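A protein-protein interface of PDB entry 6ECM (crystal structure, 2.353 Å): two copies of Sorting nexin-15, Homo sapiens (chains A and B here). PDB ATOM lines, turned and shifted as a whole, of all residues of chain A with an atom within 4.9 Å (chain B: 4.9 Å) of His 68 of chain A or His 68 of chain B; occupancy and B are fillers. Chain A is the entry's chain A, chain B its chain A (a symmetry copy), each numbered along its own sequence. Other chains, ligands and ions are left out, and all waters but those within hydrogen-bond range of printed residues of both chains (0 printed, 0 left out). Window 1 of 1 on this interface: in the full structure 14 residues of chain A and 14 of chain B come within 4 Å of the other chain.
ND1 of His 68 of chain B is in hydrogen-bond range of ND1 of His 68 of chain A, at 3.3 Å.
The side-chain hydroxyl (OH) of Tyr 66 of chain A sits close to the guanidinium group (NH2) of Arg 69 of chain A (3.4 Å). OH of Tyr 66 of chain B lies close to NH2 of Arg 69 of chain B (3.4 Å).
Among the printed residues, merely in contact across the chains: Leu 64 of chain A with Leu 75 of chain B (3.6 Å), Ala 65 of chain A with Phe 72 of chain B (3.3 Å), Ala 65 of chain A with Leu 75 of chain B (3.6 Å), His 68 of chain A with Leu 71 of chain B (3.4 Å), His 68 of chain A with Leu 75 of chain B (3.98 Å), Arg 69 of chain A with Phe 72 of chain B (3.3 Å), Leu 71 of chain A with His 68 of chain B (3.4 Å), Leu 71 of chain A with Ala 114 of chain B (3.6 Å), Phe 72 of chain A with Ala 65 of chain B (3.3 Å), Phe 72 of chain A with Arg 69 of chain B (3.3 Å), Leu 75 of chain A with Leu 64 of chain B (3.6 Å), Leu 75 of chain A with Ala 65 of chain B (3.6 Å), Leu 75 of chain A with His 68 of chain B (3.98 Å), Ala 114 of chain A with Leu 71 of chain B (3.6 Å) and Ala 114 of chain A with Ala 114 of chain B (3.9 Å).
Of the printed residues of chain B, Leu 75 of chain A touches Leu 64, Ala 65 and His 68. Of the printed residues of chain A, His 68 of chain B touches His 68 (3.3 Å), Leu 71 (3.4 Å) and Leu 75 (3.98 Å). Of the printed residues of chain A, Leu 71 of chain B touches His 68 and Ala 114. Printed residues of chain A within 4 Å of Leu 75 of chain B: Leu 64, Ala 65 and His 68. The nearest printed residue of chain B that does not touch His 68 of chain A is Phe 72 of chain B (4.3 Å).
Of the 12 printed residues of chain A, 8 touch a printed residue of chain B. Printed residues of chain A that touch a printed residue of chain B: Leu 64, Ala 65, His 68, Arg 69, Leu 71, Phe 72, Leu 75 and Ala 114. Hydrophobic or aromatic side chains of chain A that line the printed part of chain B: Leu 64, His 68, Leu 71, Phe 72, Leu 75 and Ala 114. Of the 12 printed residues of chain B, 8 touch a printed residue of chain A. Printed residues of chain B that touch a printed residue of chain A: Leu 64, Ala 65, His 68, Arg 69, Leu 71, Phe 72, Leu 75 and Ala 114. Hydrophobic or aromatic side chains of chain B within 4 Å of the printed part of chain A: Leu 64, His 68, Leu 71, Phe 72, Leu 75 and Ala 114.
Leu 64 of chain A touches Leu 75 of chain B, and with the chains exchanged Leu 75 of chain A touches Leu 64 of chain B. Ala 65 of chain A touches Leu 75 of chain B, and with the chains exchanged Leu 75 of chain A touches Ala 65 of chain B. His 68 of chain A touches Leu 75 of chain B, and with the chains exchanged Leu 75 of chain A touches His 68 of chain B. Arg 69 of chain A touches Phe 72 of chain B, and with the chains exchanged Phe 72 of chain A touches Arg 69 of chain B. Positions printed for both chains: 64, 65, 66, 67, 68, 69, 70, 71, 72, 75, 114 and 115. Of the 16 pairs that touch across the chains among the printed residues, 16 have their exchanged pair printed and touching as well.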
ATOM      1  N   LEU A  64      22.327  15.091  32.091  1.00  0.00           N
ATOM      2  CA  LEU A  64      23.728  14.896  31.772  1.00  0.00           C
ATOM      3  C   LEU A  64      23.859  13.844  30.660  1.00  0.00           C
ATOM      4  O   LEU A  64      24.459  14.112  29.603  1.00  0.00           O
ATOM      5  CB  LEU A  64      24.494  14.494  33.029  1.00  0.00           C
ATOM      6  CG  LEU A  64      24.472  15.583  34.103  1.00  0.00           C
ATOM      7  CD1 LEU A  64      25.068  15.070  35.407  1.00  0.00           C
ATOM      8  CD2 LEU A  64      25.220  16.820  33.609  1.00  0.00           C
ATOM      9  N   ALA A  65      23.253  12.676  30.883  1.00  0.00           N
ATOM     10  CA  ALA A  65      23.307  11.587  29.908  1.00  0.00           C
ATOM     11  C   ALA A  65      22.782  12.021  28.531  1.00  0.00           C
ATOM     12  O   ALA A  65      23.417  11.736  27.508  1.00  0.00           O
ATOM     13  CB  ALA A  65      22.533  10.380  30.417  1.00  0.00           C
ATOM     14  N   TYR A  66      21.649  12.723  28.492  1.00  0.00           N
ATOM     15  CA  TYR A  66      21.118  13.166  27.197  1.00  0.00           C
ATOM     16  C   TYR A  66      21.955  14.289  26.553  1.00  0.00           C
ATOM     17  O   TYR A  66      22.088  14.336  25.316  1.00  0.00           O
ATOM     18  CB  TYR A  66      19.650  13.603  27.335  1.00  0.00           C
ATOM     19  CG  TYR A  66      18.668  12.550  26.837  1.00  0.00           C
ATOM     20  CD1 TYR A  66      18.651  11.269  27.390  1.00  0.00           C
ATOM     21  CD2 TYR A  66      17.771  12.828  25.808  1.00  0.00           C
ATOM     22  CE1 TYR A  66      17.764  10.295  26.937  1.00  0.00           C
ATOM     23  CE2 TYR A  66      16.875  11.858  25.349  1.00  0.00           C
ATOM     24  CZ  TYR A  66      16.879  10.594  25.920  1.00  0.00           C
ATOM     25  OH  TYR A  66      15.999   9.627  25.475  1.00  0.00           O
ATOM     26  N   THR A  67      22.520  15.181  27.368  1.00  0.00           N
ATOM     27  CA  THR A  67      23.389  16.234  26.830  1.00  0.00           C
ATOM     28  C   THR A  67      24.618  15.627  26.133  1.00  0.00           C
ATOM     29  O   THR A  67      25.033  16.076  25.058  1.00  0.00           O
ATOM     30  CB  THR A  67      23.878  17.221  27.924  1.00  0.00           C
ATOM     31  OG1 THR A  67      22.752  17.816  28.590  1.00  0.00           O
ATOM     32  CG2 THR A  67      24.717  18.332  27.307  1.00  0.00           C
ATOM     33  N   HIS A  68      25.202  14.597  26.733  1.00  0.00           N
ATOM     34  CA  HIS A  68      26.410  14.039  26.146  1.00  0.00           C
ATOM     35  C   HIS A  68      26.097  13.088  24.999  1.00  0.00           C
ATOM     36  O   HIS A  68      26.882  12.984  24.050  1.00  0.00           O
ATOM     37  CB  HIS A  68      27.251  13.357  27.220  1.00  0.00           C
ATOM     38  CG  HIS A  68      27.887  14.326  28.165  1.00  0.00           C
ATOM     39  ND1 HIS A  68      29.156  14.830  27.971  1.00  0.00           N
ATOM     40  CD2 HIS A  68      27.410  14.920  29.284  1.00  0.00           C
ATOM     41  CE1 HIS A  68      29.439  15.681  28.940  1.00  0.00           C
ATOM     42  NE2 HIS A  68      28.397  15.754  29.750  1.00  0.00           N
ATOM     43  N   ARG A  69      24.945  12.421  25.065  1.00  0.00           N
ATOM     44  CA  ARG A  69      24.489  11.605  23.944  1.00  0.00           C
ATOM     45  C   ARG A  69      24.314  12.479  22.707  1.00  0.00           C
ATOM     46  O   ARG A  69      24.759  12.130  21.605  1.00  0.00           O
ATOM     47  CB  ARG A  69      23.174  10.884  24.268  1.00  0.00           C
ATOM     48  CG  ARG A  69      22.949   9.607  23.443  1.00  0.00           C
ATOM     49  CD  ARG A  69      21.959   9.791  22.296  1.00  0.00           C
ATOM     50  NE  ARG A  69      20.574   9.533  22.690  1.00  0.00           N
ATOM     51  CZ  ARG A  69      19.622  10.461  22.732  1.00  0.00           C
ATOM     52  NH1 ARG A  69      19.902  11.715  22.400  1.00  0.00           N
ATOM     53  NH2 ARG A  69      18.389  10.136  23.101  1.00  0.00           N
ATOM     54  N   ASN A  70      23.673  13.626  22.891  1.00  0.00           N
ATOM     55  CA  ASN A  70      23.427  14.500  21.753  1.00  0.00           C
ATOM     56  C   ASN A  70      24.679  15.262  21.318  1.00  0.00           C
ATOM     57  O   ASN A  70      24.818  15.608  20.141  1.00  0.00           O
ATOM     58  CB  ASN A  70      22.282  15.467  22.062  1.00  0.00           C
ATOM     59  CG  ASN A  70      20.928  14.924  21.608  1.00  0.00           C
ATOM     60  OD1 ASN A  70      20.423  13.933  22.148  1.00  0.00           O
ATOM     61  ND2 ASN A  70      20.338  15.572  20.606  1.00  0.00           N
ATOM     62  N   LEU A  71      25.590  15.516  22.254  1.00  0.00           N
ATOM     63  CA  LEU A  71      26.863  16.119  21.888  1.00  0.00           C
ATOM     64  C   LEU A  71      27.566  15.164  20.951  1.00  0.00           C
ATOM     65  O   LEU A  71      28.092  15.555  19.916  1.00  0.00           O
ATOM     66  CB  LEU A  71      27.734  16.402  23.112  1.00  0.00           C
ATOM     67  CG  LEU A  71      28.212  17.849  23.221  1.00  0.00           C
ATOM     68  CD1 LEU A  71      27.008  18.761  23.273  1.00  0.00           C
ATOM     69  CD2 LEU A  71      29.074  18.052  24.447  1.00  0.00           C
ATOM     70  N   PHE A  72      27.548  13.895  21.326  1.00  0.00           N
ATOM     71  CA  PHE A  72      28.146  12.848  20.521  1.00  0.00           C
ATOM     72  C   PHE A  72      27.519  12.772  19.126  1.00  0.00           C
ATOM     73  O   PHE A  72      28.220  12.826  18.096  1.00  0.00           O
ATOM     74  CB  PHE A  72      28.004  11.520  21.254  1.00  0.00           C
ATOM     75  CG  PHE A  72      28.162  10.336  20.377  1.00  0.00           C
ATOM     76  CD1 PHE A  72      27.056   9.604  19.983  1.00  0.00           C
ATOM     77  CD2 PHE A  72      29.416   9.954  19.939  1.00  0.00           C
ATOM     78  CE1 PHE A  72      27.201   8.505  19.164  1.00  0.00           C
ATOM     79  CE2 PHE A  72      29.571   8.859  19.116  1.00  0.00           C
ATOM     80  CZ  PHE A  72      28.465   8.128  18.731  1.00  0.00           C
ATOM     81  N   LEU A  75      28.652  15.794  17.108  1.00  0.00           N
ATOM     82  CA  LEU A  75      30.040  15.727  16.673  1.00  0.00           C
ATOM     83  C   LEU A  75      30.116  14.833  15.454  1.00  0.00           C
ATOM     84  O   LEU A  75      30.702  15.199  14.439  1.00  0.00           O
ATOM     85  CB  LEU A  75      30.951  15.203  17.789  1.00  0.00           C
ATOM     86  CG  LEU A  75      31.080  16.139  18.993  1.00  0.00           C
ATOM     87  CD1 LEU A  75      31.865  15.477  20.117  1.00  0.00           C
ATOM     88  CD2 LEU A  75      31.724  17.457  18.578  1.00  0.00           C
ATOM     89  N   ALA A 114      34.312  17.936  31.455  1.00  0.00           N
ATOM     90  CA  ALA A 114      33.156  17.952  30.573  1.00  0.00           C
ATOM     91  C   ALA A 114      31.897  17.986  31.421  1.00  0.00           C
ATOM     92  O   ALA A 114      30.932  18.660  31.078  1.00  0.00           O
ATOM     93  CB  ALA A 114      33.152  16.742  29.644  1.00  0.00           C
ATOM     94  N   LEU A 115      31.935  17.276  32.544  1.00  0.00           N
ATOM     95  CA  LEU A 115      30.832  17.261  33.498  1.00  0.00           C
ATOM     96  C   LEU A 115      30.933  18.410  34.510  1.00  0.00           C
ATOM     97  O   LEU A 115      29.947  19.061  34.801  1.00  0.00           O
ATOM     98  CB  LEU A 115      30.789  15.914  34.220  1.00  0.00           C
ATOM     99  CG  LEU A 115      30.406  14.738  33.321  1.00  0.00           C
ATOM    100  CD1 LEU A 115      30.511  13.403  34.054  1.00  0.00           C
ATOM    101  CD2 LEU A 115      28.996  14.941  32.786  1.00  0.00           C
ATOM    102  N   LEU B  64      37.169  13.813  20.495  1.00  0.00           N
ATOM    103  CA  LEU B  64      36.024  14.476  21.090  1.00  0.00           C
ATOM    104  C   LEU B  64      34.804  13.545  21.026  1.00  0.00           C
ATOM    105  O   LEU B  64      34.184  13.241  22.061  1.00  0.00           O
ATOM    106  CB  LEU B  64      35.767  15.803  20.383  1.00  0.00           C
ATOM    107  CG  LEU B  64      36.929  16.786  20.539  1.00  0.00           C
ATOM    108  CD1 LEU B  64      36.724  18.011  19.658  1.00  0.00           C
ATOM    109  CD2 LEU B  64      37.082  17.186  22.005  1.00  0.00           C
ATOM    110  N   ALA B  65      34.499  13.059  19.821  1.00  0.00           N
ATOM    111  CA  ALA B  65      33.357  12.168  19.621  1.00  0.00           C
ATOM    112  C   ALA B  65      33.435  10.922  20.515  1.00  0.00           C
ATOM    113  O   ALA B  65      32.440  10.550  21.149  1.00  0.00           O
ATOM    114  CB  ALA B  65      33.247  11.767  18.156  1.00  0.00           C
ATOM    115  N   TYR B  66      34.605  10.287  20.594  1.00  0.00           N
ATOM    116  CA  TYR B  66      34.726   9.098  21.446  1.00  0.00           C
ATOM    117  C   TYR B  66      34.687   9.425  22.951  1.00  0.00           C
ATOM    118  O   TYR B  66      34.146   8.636  23.747  1.00  0.00           O
ATOM    119  CB  TYR B  66      36.002   8.312  21.101  1.00  0.00           C
ATOM    120  CG  TYR B  66      35.728   7.082  20.244  1.00  0.00           C
ATOM    121  CD1 TYR B  66      35.107   7.201  19.001  1.00  0.00           C
ATOM    122  CD2 TYR B  66      36.077   5.806  20.680  1.00  0.00           C
ATOM    123  CE1 TYR B  66      34.843   6.083  18.212  1.00  0.00           C
ATOM    124  CE2 TYR B  66      35.819   4.679  19.894  1.00  0.00           C
ATOM    125  CZ  TYR B  66      35.202   4.827  18.660  1.00  0.00           C
ATOM    126  OH  TYR B  66      34.942   3.721  17.875  1.00  0.00           O
ATOM    127  N   THR B  67      35.243  10.572  23.346  1.00  0.00           N
ATOM    128  CA  THR B  67      35.178  10.983  24.754  1.00  0.00           C
ATOM    129  C   THR B  67      33.720  11.173  25.203  1.00  0.00           C
ATOM    130  O   THR B  67      33.332  10.771  26.306  1.00  0.00           O
ATOM    131  CB  THR B  67      35.956  12.299  25.027  1.00  0.00           C
ATOM    132  OG1 THR B  67      37.329  12.153  24.627  1.00  0.00           O
ATOM    133  CG2 THR B  67      35.919  12.645  26.510  1.00  0.00           C
ATOM    134  N   HIS B  68      32.903  11.777  24.350  1.00  0.00           N
ATOM    135  CA  HIS B  68      31.534  12.043  24.764  1.00  0.00           C
ATOM    136  C   HIS B  68      30.648  10.813  24.616  1.00  0.00           C
ATOM    137  O   HIS B  68      29.706  10.632  25.396  1.00  0.00           O
ATOM    138  CB  HIS B  68      30.971  13.230  23.990  1.00  0.00           C
ATOM    139  CG  HIS B  68      31.584  14.532  24.393  1.00  0.00           C
ATOM    140  ND1 HIS B  68      31.037  15.342  25.367  1.00  0.00           N
ATOM    141  CD2 HIS B  68      32.723  15.142  23.989  1.00  0.00           C
ATOM    142  CE1 HIS B  68      31.805  16.403  25.533  1.00  0.00           C
ATOM    143  NE2 HIS B  68      32.835  16.306  24.709  1.00  0.00           N
ATOM    144  N   ARG B  69      30.961   9.956  23.646  1.00  0.00           N
ATOM    145  CA  ARG B  69      30.265   8.678  23.523  1.00  0.00           C
ATOM    146  C   ARG B  69      30.470   7.856  24.792  1.00  0.00           C
ATOM    147  O   ARG B  69      29.521   7.289  25.350  1.00  0.00           O
ATOM    148  CB  ARG B  69      30.749   7.886  22.301  1.00  0.00           C
ATOM    149  CG  ARG B  69      29.717   6.879  21.769  1.00  0.00           C
ATOM    150  CD  ARG B  69      30.016   5.436  22.170  1.00  0.00           C
ATOM    151  NE  ARG B  69      30.878   4.745  21.211  1.00  0.00           N
ATOM    152  CZ  ARG B  69      32.115   4.336  21.477  1.00  0.00           C
ATOM    153  NH1 ARG B  69      32.640   4.545  22.679  1.00  0.00           N
ATOM    154  NH2 ARG B  69      32.828   3.713  20.546  1.00  0.00           N
ATOM    155  N   ASN B  70      31.711   7.802  25.256  1.00  0.00           N
ATOM    156  CA  ASN B  70      31.999   7.003  26.439  1.00  0.00           C
ATOM    157  C   ASN B  70      31.540   7.683  27.729  1.00  0.00           C
ATOM    158  O   ASN B  70      31.217   7.003  28.708  1.00  0.00           O
ATOM    159  CB  ASN B  70      33.490   6.666  26.504  1.00  0.00           C
ATOM    160  CG  ASN B  70      33.809   5.327  25.841  1.00  0.00           C
ATOM    161  OD1 ASN B  70      33.685   5.173  24.620  1.00  0.00           O
ATOM    162  ND2 ASN B  70      34.219   4.351  26.648  1.00  0.00           N
ATOM    163  N   LEU B  71      31.500   9.013  27.734  1.00  0.00           N
ATOM    164  CA  LEU B  71      30.948   9.722  28.879  1.00  0.00           C
ATOM    165  C   LEU B  71      29.498   9.318  29.009  1.00  0.00           C
ATOM    166  O   LEU B  71      29.016   9.006  30.091  1.00  0.00           O
ATOM    167  CB  LEU B  71      31.066  11.238  28.723  1.00  0.00           C
ATOM    168  CG  LEU B  71      31.768  11.936  29.888  1.00  0.00           C
ATOM    169  CD1 LEU B  71      33.159  11.363  30.037  1.00  0.00           C
ATOM    170  CD2 LEU B  71      31.839  13.430  29.669  1.00  0.00           C
ATOM    171  N   PHE B  72      28.814   9.310  27.876  1.00  0.00           N
ATOM    172  CA  PHE B  72      27.421   8.912  27.823  1.00  0.00           C
ATOM    173  C   PHE B  72      27.218   7.478  28.322  1.00  0.00           C
ATOM    174  O   PHE B  72      26.402   7.216  29.228  1.00  0.00           O
ATOM    175  CB  PHE B  72      26.918   9.066  26.393  1.00  0.00           C
ATOM    176  CG  PHE B  72      25.684   8.295  26.109  1.00  0.00           C
ATOM    177  CD1 PHE B  72      25.744   7.124  25.374  1.00  0.00           C
ATOM    178  CD2 PHE B  72      24.462   8.735  26.582  1.00  0.00           C
ATOM    179  CE1 PHE B  72      24.598   6.405  25.112  1.00  0.00           C
ATOM    180  CE2 PHE B  72      23.311   8.019  26.330  1.00  0.00           C
ATOM    181  CZ  PHE B  72      23.375   6.854  25.589  1.00  0.00           C
ATOM    182  N   LEU B  75      27.711   7.413  32.095  1.00  0.00           N
ATOM    183  CA  LEU B  75      26.614   8.010  32.845  1.00  0.00           C
ATOM    184  C   LEU B  75      25.491   6.999  32.933  1.00  0.00           C
ATOM    185  O   LEU B  75      24.961   6.737  34.010  1.00  0.00           O
ATOM    186  CB  LEU B  75      26.129   9.307  32.188  1.00  0.00           C
ATOM    187  CG  LEU B  75      27.144  10.452  32.219  1.00  0.00           C
ATOM    188  CD1 LEU B  75      26.649  11.642  31.409  1.00  0.00           C
ATOM    189  CD2 LEU B  75      27.447  10.857  33.657  1.00  0.00           C
ATOM    190  N   ALA B 114      31.205  21.916  27.630  1.00  0.00           N
ATOM    191  CA  ALA B 114      31.600  20.518  27.692  1.00  0.00           C
ATOM    192  C   ALA B 114      32.756  20.297  26.733  1.00  0.00           C
ATOM    193  O   ALA B 114      33.682  19.550  27.032  1.00  0.00           O
ATOM    194  CB  ALA B 114      30.432  19.596  27.356  1.00  0.00           C
ATOM    195  N   LEU B 115      32.704  20.980  25.593  1.00  0.00           N
ATOM    196  CA  LEU B 115      33.770  20.928  24.600  1.00  0.00           C
ATOM    197  C   LEU B 115      34.868  21.961  24.883  1.00  0.00           C
ATOM    198  O   LEU B 115      36.042  21.650  24.794  1.00  0.00           O
ATOM    199  CB  LEU B 115      33.187  21.136  23.202  1.00  0.00           C
ATOM    200  CG  LEU B 115      32.293  19.992  22.723  1.00  0.00           C
ATOM    201  CD1 LEU B 115      31.629  20.309  21.387  1.00  0.00           C
ATOM    202  CD2 LEU B 115      33.112  18.713  22.619  1.00  0.00           C
